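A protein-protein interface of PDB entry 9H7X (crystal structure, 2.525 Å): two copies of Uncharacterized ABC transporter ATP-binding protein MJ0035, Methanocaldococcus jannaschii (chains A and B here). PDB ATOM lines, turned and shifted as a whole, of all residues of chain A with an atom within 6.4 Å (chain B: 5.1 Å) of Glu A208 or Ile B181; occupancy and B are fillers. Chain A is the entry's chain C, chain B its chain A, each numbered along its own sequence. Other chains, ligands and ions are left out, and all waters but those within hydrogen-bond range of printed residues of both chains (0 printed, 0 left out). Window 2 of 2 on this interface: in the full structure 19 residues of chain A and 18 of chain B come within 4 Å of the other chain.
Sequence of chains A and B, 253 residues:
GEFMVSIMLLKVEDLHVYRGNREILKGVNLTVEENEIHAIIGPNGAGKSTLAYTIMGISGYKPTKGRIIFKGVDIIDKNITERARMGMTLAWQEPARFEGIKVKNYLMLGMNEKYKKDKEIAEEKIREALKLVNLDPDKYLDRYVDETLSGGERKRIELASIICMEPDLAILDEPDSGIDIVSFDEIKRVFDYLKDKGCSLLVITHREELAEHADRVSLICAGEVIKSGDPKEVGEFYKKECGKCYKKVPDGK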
ATOM      1  N   THR A 205     -27.029  -5.324 -19.713  1.00  0.00           N
ATOM      2  CA  THR A 205     -26.244  -5.623 -18.517  1.00  0.00           C
ATOM      3  C   THR A 205     -25.800  -7.074 -18.400  1.00  0.00           C
ATOM      4  O   THR A 205     -26.437  -7.982 -18.933  1.00  0.00           O
ATOM      5  CB  THR A 205     -26.998  -5.173 -17.246  1.00  0.00           C
ATOM      6  OG1 THR A 205     -26.145  -5.353 -16.123  1.00  0.00           O
ATOM      7  CG2 THR A 205     -28.304  -5.911 -17.038  1.00  0.00           C
ATOM      8  N   HIS A 206     -24.670  -7.270 -17.697  1.00  0.00           N
ATOM      9  CA  HIS A 206     -24.107  -8.575 -17.336  1.00  0.00           C
ATOM     10  C   HIS A 206     -24.286  -8.882 -15.826  1.00  0.00           C
ATOM     11  O   HIS A 206     -23.960  -9.987 -15.381  1.00  0.00           O
ATOM     12  CB  HIS A 206     -22.645  -8.727 -17.784  1.00  0.00           C
ATOM     13  CG  HIS A 206     -22.506  -8.996 -19.254  1.00  0.00           C
ATOM     14  ND1 HIS A 206     -21.956  -8.073 -20.117  1.00  0.00           N
ATOM     15  CD2 HIS A 206     -22.872 -10.087 -19.960  1.00  0.00           C
ATOM     16  CE1 HIS A 206     -22.004  -8.631 -21.315  1.00  0.00           C
ATOM     17  NE2 HIS A 206     -22.556  -9.835 -21.269  1.00  0.00           N
ATOM     18  N   ARG A 207     -24.853  -7.928 -15.054  1.00  0.00           N
ATOM     19  CA  ARG A 207     -25.126  -8.086 -13.642  1.00  0.00           C
ATOM     20  C   ARG A 207     -26.557  -8.546 -13.441  1.00  0.00           C
ATOM     21  O   ARG A 207     -27.481  -7.801 -13.738  1.00  0.00           O
ATOM     22  CB  ARG A 207     -24.916  -6.759 -12.909  1.00  0.00           C
ATOM     23  CG  ARG A 207     -23.461  -6.342 -12.789  1.00  0.00           C
ATOM     24  CD  ARG A 207     -22.661  -7.318 -11.952  1.00  0.00           C
ATOM     25  NE  ARG A 207     -21.356  -6.773 -11.581  1.00  0.00           N
ATOM     26  CZ  ARG A 207     -20.551  -7.305 -10.670  1.00  0.00           C
ATOM     27  NH1 ARG A 207     -20.906  -8.406 -10.022  1.00  0.00           N
ATOM     28  NH2 ARG A 207     -19.385  -6.734 -10.395  1.00  0.00           N
ATOM     29  N   GLU A 208     -26.752  -9.756 -12.899  1.00  0.00           N
ATOM     30  CA  GLU A 208     -28.097 -10.251 -12.585  1.00  0.00           C
ATOM     31  C   GLU A 208     -28.771  -9.338 -11.552  1.00  0.00           C
ATOM     32  O   GLU A 208     -29.978  -9.156 -11.593  1.00  0.00           O
ATOM     33  CB  GLU A 208     -28.025 -11.663 -12.011  1.00  0.00           C
ATOM     34  CG  GLU A 208     -27.291 -12.664 -12.883  1.00  0.00           C
ATOM     35  CD  GLU A 208     -26.927 -13.920 -12.115  1.00  0.00           C
ATOM     36  OE1 GLU A 208     -27.797 -14.814 -11.992  1.00  0.00           O
ATOM     37  OE2 GLU A 208     -25.781 -13.993 -11.611  1.00  0.00           O
ATOM     38  N   GLU A 209     -27.972  -8.734 -10.647  1.00  0.00           N
ATOM     39  CA  GLU A 209     -28.374  -7.779  -9.618  1.00  0.00           C
ATOM     40  C   GLU A 209     -29.201  -6.654 -10.261  1.00  0.00           C
ATOM     41  O   GLU A 209     -30.270  -6.329  -9.766  1.00  0.00           O
ATOM     42  CB  GLU A 209     -27.111  -7.193  -8.930  1.00  0.00           C
ATOM     43  CG  GLU A 209     -26.231  -8.216  -8.224  1.00  0.00           C
ATOM     44  CD  GLU A 209     -25.092  -8.854  -9.009  1.00  0.00           C
ATOM     45  OE1 GLU A 209     -25.222  -8.992 -10.247  1.00  0.00           O
ATOM     46  OE2 GLU A 209     -24.075  -9.237  -8.382  1.00  0.00           O
ATOM     47  N   LEU A 210     -28.743  -6.134 -11.412  1.00  0.00           N
ATOM     48  CA  LEU A 210     -29.425  -5.073 -12.138  1.00  0.00           C
ATOM     49  C   LEU A 210     -30.493  -5.580 -13.092  1.00  0.00           C
ATOM     50  O   LEU A 210     -31.551  -4.964 -13.194  1.00  0.00           O
ATOM     51  CB  LEU A 210     -28.420  -4.207 -12.917  1.00  0.00           C
ATOM     52  CG  LEU A 210     -27.658  -3.115 -12.160  1.00  0.00           C
ATOM     53  CD1 LEU A 210     -27.037  -2.148 -13.141  1.00  0.00           C
ATOM     54  CD2 LEU A 210     -28.579  -2.319 -11.217  1.00  0.00           C
ATOM     55  N   ALA A 211     -30.224  -6.674 -13.811  1.00  0.00           N
ATOM     56  CA  ALA A 211     -31.194  -7.231 -14.748  1.00  0.00           C
ATOM     57  C   ALA A 211     -32.476  -7.691 -14.034  1.00  0.00           C
ATOM     58  O   ALA A 211     -33.561  -7.542 -14.584  1.00  0.00           O
ATOM     59  CB  ALA A 211     -30.573  -8.375 -15.531  1.00  0.00           C
ATOM     60  N   GLU A 212     -32.368  -8.198 -12.797  1.00  0.00           N
ATOM     61  CA  GLU A 212     -33.547  -8.594 -12.029  1.00  0.00           C
ATOM     62  C   GLU A 212     -34.352  -7.396 -11.489  1.00  0.00           C
ATOM     63  O   GLU A 212     -35.477  -7.582 -11.026  1.00  0.00           O
ATOM     64  CB  GLU A 212     -33.193  -9.584 -10.921  1.00  0.00           C
ATOM     65  CG  GLU A 212     -32.743 -10.930 -11.467  1.00  0.00           C
ATOM     66  CD  GLU A 212     -32.178 -11.890 -10.431  1.00  0.00           C
ATOM     67  OE1 GLU A 212     -32.534 -11.758  -9.238  1.00  0.00           O
ATOM     68  OE2 GLU A 212     -31.366 -12.769 -10.810  1.00  0.00           O
ATOM     69  N   HIS A 213     -33.799  -6.175 -11.569  1.00  0.00           N
ATOM     70  CA  HIS A 213     -34.480  -4.940 -11.166  1.00  0.00           C
ATOM     71  C   HIS A 213     -35.417  -4.397 -12.269  1.00  0.00           C
ATOM     72  O   HIS A 213     -36.304  -3.605 -11.978  1.00  0.00           O
ATOM     73  CB  HIS A 213     -33.458  -3.872 -10.765  1.00  0.00           C
ATOM     74  CG  HIS A 213     -34.062  -2.710 -10.049  1.00  0.00           C
ATOM     75  ND1 HIS A 213     -34.489  -2.812  -8.735  1.00  0.00           N
ATOM     76  CD2 HIS A 213     -34.284  -1.452 -10.487  1.00  0.00           C
ATOM     77  CE1 HIS A 213     -34.952  -1.614  -8.417  1.00  0.00           C
ATOM     78  NE2 HIS A 213     -34.850  -0.764  -9.440  1.00  0.00           N
ATOM     79  N   GLY A 235     -33.371 -14.992 -16.861  1.00  0.00           N
ATOM     80  CA  GLY A 235     -32.008 -15.044 -16.350  1.00  0.00           C
ATOM     81  C   GLY A 235     -31.553 -16.466 -16.112  1.00  0.00           C
ATOM     82  O   GLY A 235     -30.431 -16.827 -16.461  1.00  0.00           O
ATOM     83  N   GLU A 236     -32.442 -17.304 -15.552  1.00  0.00           N
ATOM     84  CA  GLU A 236     -32.132 -18.710 -15.299  1.00  0.00           C
ATOM     85  C   GLU A 236     -31.987 -19.509 -16.588  1.00  0.00           C
ATOM     86  O   GLU A 236     -31.101 -20.351 -16.690  1.00  0.00           O
ATOM     87  CB  GLU A 236     -33.143 -19.349 -14.338  1.00  0.00           C
ATOM     88  CG  GLU A 236     -32.929 -18.953 -12.883  1.00  0.00           C
ATOM     89  CD  GLU A 236     -31.504 -19.097 -12.374  1.00  0.00           C
ATOM     90  OE1 GLU A 236     -31.040 -20.251 -12.206  1.00  0.00           O
ATOM     91  OE2 GLU A 236     -30.842 -18.053 -12.168  1.00  0.00           O
ATOM     92  N   TYR A 238     -30.838 -18.288 -19.368  1.00  0.00           N
ATOM     93  CA  TYR A 238     -29.559 -17.848 -19.929  1.00  0.00           C
ATOM     94  C   TYR A 238     -28.416 -18.640 -19.310  1.00  0.00           C
ATOM     95  O   TYR A 238     -27.618 -19.235 -20.030  1.00  0.00           O
ATOM     96  CB  TYR A 238     -29.377 -16.323 -19.729  1.00  0.00           C
ATOM     97  CG  TYR A 238     -27.981 -15.789 -19.985  1.00  0.00           C
ATOM     98  CD1 TYR A 238     -27.442 -15.776 -21.264  1.00  0.00           C
ATOM     99  CD2 TYR A 238     -27.232 -15.228 -18.961  1.00  0.00           C
ATOM    100  CE1 TYR A 238     -26.166 -15.271 -21.505  1.00  0.00           C
ATOM    101  CE2 TYR A 238     -25.957 -14.721 -19.189  1.00  0.00           C
ATOM    102  CZ  TYR A 238     -25.426 -14.745 -20.463  1.00  0.00           C
ATOM    103  OH  TYR A 238     -24.162 -14.257 -20.678  1.00  0.00           O
ATOM    104  N   LYS A 239     -28.401 -18.720 -17.965  1.00  0.00           N
ATOM    105  CA  LYS A 239     -27.393 -19.436 -17.177  1.00  0.00           C
ATOM    106  C   LYS A 239     -27.418 -20.958 -17.357  1.00  0.00           C
ATOM    107  O   LYS A 239     -26.642 -21.653 -16.693  1.00  0.00           O
ATOM    108  CB  LYS A 239     -27.582 -19.140 -15.686  1.00  0.00           C
ATOM    109  CG  LYS A 239     -27.498 -17.683 -15.312  1.00  0.00           C
ATOM    110  CD  LYS A 239     -27.797 -17.502 -13.842  1.00  0.00           C
ATOM    111  CE  LYS A 239     -26.688 -18.062 -12.979  1.00  0.00           C
ATOM    112  NZ  LYS A 239     -26.861 -17.719 -11.542  1.00  0.00           N
ATOM    113  N   ILE B 179     -17.023  -9.056 -20.183  1.00  0.00           N
ATOM    114  CA  ILE B 179     -17.140 -10.465 -20.507  1.00  0.00           C
ATOM    115  C   ILE B 179     -18.401 -11.040 -19.854  1.00  0.00           C
ATOM    116  O   ILE B 179     -18.729 -10.695 -18.717  1.00  0.00           O
ATOM    117  CB  ILE B 179     -15.829 -11.217 -20.179  1.00  0.00           C
ATOM    118  CG1 ILE B 179     -14.763 -10.900 -21.252  1.00  0.00           C
ATOM    119  CG2 ILE B 179     -16.044 -12.728 -20.053  1.00  0.00           C
ATOM    120  CD1 ILE B 179     -13.402 -11.330 -20.908  1.00  0.00           C
ATOM    121  N   ASP B 180     -19.158 -11.838 -20.611  1.00  0.00           N
ATOM    122  CA  ASP B 180     -20.391 -12.439 -20.126  1.00  0.00           C
ATOM    123  C   ASP B 180     -20.133 -13.462 -19.019  1.00  0.00           C
ATOM    124  O   ASP B 180     -19.077 -14.079 -19.008  1.00  0.00           O
ATOM    125  CB  ASP B 180     -21.165 -13.076 -21.293  1.00  0.00           C
ATOM    126  CG  ASP B 180     -20.402 -14.140 -22.055  1.00  0.00           C
ATOM    127  OD1 ASP B 180     -19.994 -15.133 -21.436  1.00  0.00           O
ATOM    128  OD2 ASP B 180     -20.249 -13.997 -23.278  1.00  0.00           O
ATOM    129  N   ILE B 181     -21.126 -13.705 -18.141  1.00  0.00           N
ATOM    130  CA  ILE B 181     -21.001 -14.639 -17.016  1.00  0.00           C
ATOM    131  C   ILE B 181     -21.015 -16.130 -17.437  1.00  0.00           C
ATOM    132  O   ILE B 181     -20.600 -16.996 -16.665  1.00  0.00           O
ATOM    133  CB  ILE B 181     -22.048 -14.336 -15.916  1.00  0.00           C
ATOM    134  CG1 ILE B 181     -23.471 -14.726 -16.347  1.00  0.00           C
ATOM    135  CG2 ILE B 181     -21.980 -12.881 -15.508  1.00  0.00           C
ATOM    136  CD1 ILE B 181     -24.559 -14.510 -15.245  1.00  0.00           C
ATOM    137  N   VAL B 182     -21.478 -16.424 -18.658  1.00  0.00           N
ATOM    138  CA  VAL B 182     -21.486 -17.784 -19.207  1.00  0.00           C
ATOM    139  C   VAL B 182     -20.060 -18.203 -19.698  1.00  0.00           C
ATOM    140  O   VAL B 182     -19.866 -19.342 -20.115  1.00  0.00           O
ATOM    141  CB  VAL B 182     -22.577 -17.892 -20.317  1.00  0.00           C
ATOM    142  CG1 VAL B 182     -22.063 -17.410 -21.666  1.00  0.00           C
ATOM    143  CG2 VAL B 182     -23.145 -19.300 -20.427  1.00  0.00           C
ATOM    144  N   SER B 183     -19.067 -17.283 -19.612  1.00  0.00           N
ATOM    145  CA  SER B 183     -17.668 -17.462 -19.994  1.00  0.00           C
ATOM    146  C   SER B 183     -16.697 -17.185 -18.847  1.00  0.00           C
ATOM    147  O   SER B 183     -15.512 -16.970 -19.114  1.00  0.00           O
ATOM    148  CB  SER B 183     -17.301 -16.543 -21.155  1.00  0.00           C
ATOM    149  OG  SER B 183     -18.087 -16.803 -22.305  1.00  0.00           O
ATOM    150  N   PHE B 184     -17.170 -17.182 -17.588  1.00  0.00           N
ATOM    151  CA  PHE B 184     -16.283 -16.951 -16.453  1.00  0.00           C
ATOM    152  C   PHE B 184     -15.385 -18.140 -16.140  1.00  0.00           C
ATOM    153  O   PHE B 184     -14.321 -17.947 -15.558  1.00  0.00           O
ATOM    154  CB  PHE B 184     -17.068 -16.489 -15.222  1.00  0.00           C
ATOM    155  CG  PHE B 184     -17.464 -15.025 -15.217  1.00  0.00           C
ATOM    156  CD1 PHE B 184     -17.103 -14.182 -16.258  1.00  0.00           C
ATOM    157  CD2 PHE B 184     -18.180 -14.490 -14.164  1.00  0.00           C
ATOM    158  CE1 PHE B 184     -17.483 -12.849 -16.257  1.00  0.00           C
ATOM    159  CE2 PHE B 184     -18.554 -13.153 -14.167  1.00  0.00           C
ATOM    160  CZ  PHE B 184     -18.198 -12.342 -15.208  1.00  0.00           C
ATOM    161  N   ARG B 207     -15.805  -8.989  -9.611  1.00  0.00           N
ATOM    162  CA  ARG B 207     -16.522 -10.243  -9.671  1.00  0.00           C
ATOM    163  C   ARG B 207     -16.030 -11.166  -8.565  1.00  0.00           C
ATOM    164  O   ARG B 207     -14.875 -11.591  -8.587  1.00  0.00           O
ATOM    165  CB  ARG B 207     -16.295 -10.923 -11.023  1.00  0.00           C
ATOM    166  CG  ARG B 207     -17.006 -10.250 -12.177  1.00  0.00           C
ATOM    167  CD  ARG B 207     -18.510 -10.305 -12.028  1.00  0.00           C
ATOM    168  NE  ARG B 207     -19.185  -9.931 -13.270  1.00  0.00           N
ATOM    169  CZ  ARG B 207     -20.484 -10.093 -13.502  1.00  0.00           C
ATOM    170  NH1 ARG B 207     -21.272 -10.621 -12.573  1.00  0.00           N
ATOM    171  NH2 ARG B 207     -21.006  -9.725 -14.665  1.00  0.00           N
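Arg A207 touches its own counterpart, Arg B207. Position printed for both chains: 207. Of the 8 pairs that touch across the chains among the printed residues, 1 has its exchanged pair printed and touching as well.
Hydrophobic or aromatic side chains of chain B within 4 Å of the printed part of chain A: Ile B181 and Val B182. Among the printed residues, 8 pairs touch across the chains.
The side-chain carboxylate of Glu A209 lies within salt-bridge range of the guanidinium group of Arg A207, at 3.7 Å. The side-chain carboxylate (OD1) of Asp B180 lies close to the backbone NH (N) of Val B182. The side-chain carboxylate of Asp B180 sits at hydrogen-bond distance from the side-chain hydroxyl of Ser B183 (2.7 Å). The side-chain hydroxyl of Thr A205 sits at hydrogen-bond distance from the backbone NH of Arg A207 (3.1 Å). The side-chain carboxylate (OE1) of Glu A208 lies within salt-bridge range of the side-chain amino group (NZ) of Lys A239, at 3.1 Å.
The backbone carbonyl oxygen (O) of His A206 sits at hydrogen-bond distance from the guanidinium group (NH2) of Arg B207, 3.1 Å away. NH1 of Arg A207 lies close to NH1 of Arg B207, at 3.4 Å.
His A206 touches Asp B180 (CD2 to CA, 3.4 Å). Ile B181 touches His A206. Glu A208 touches Ile B181. CB of Asp B180 touches OH of Tyr A238, at 3.3 Å. CE2 of Tyr A238 touches CG1 of Ile B181 (3.8 Å). OH of Tyr A238 touches CG1 of Val B182, 3.9 Å away.
Glu A208 touches one residue of chain B. Ile B181 touches three residues of chain A. Printed residues of chain A within 4 Å of Val B182: Tyr A238. Of the printed residues of chain B, His A206 touches Asp B180 (3.4 Å), Ile B181 (3.5 Å) and Arg B207 (3.1 Å). The nearest residue of chain A that does not touch Ile B181 is Lys A239 (4.3 Å).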
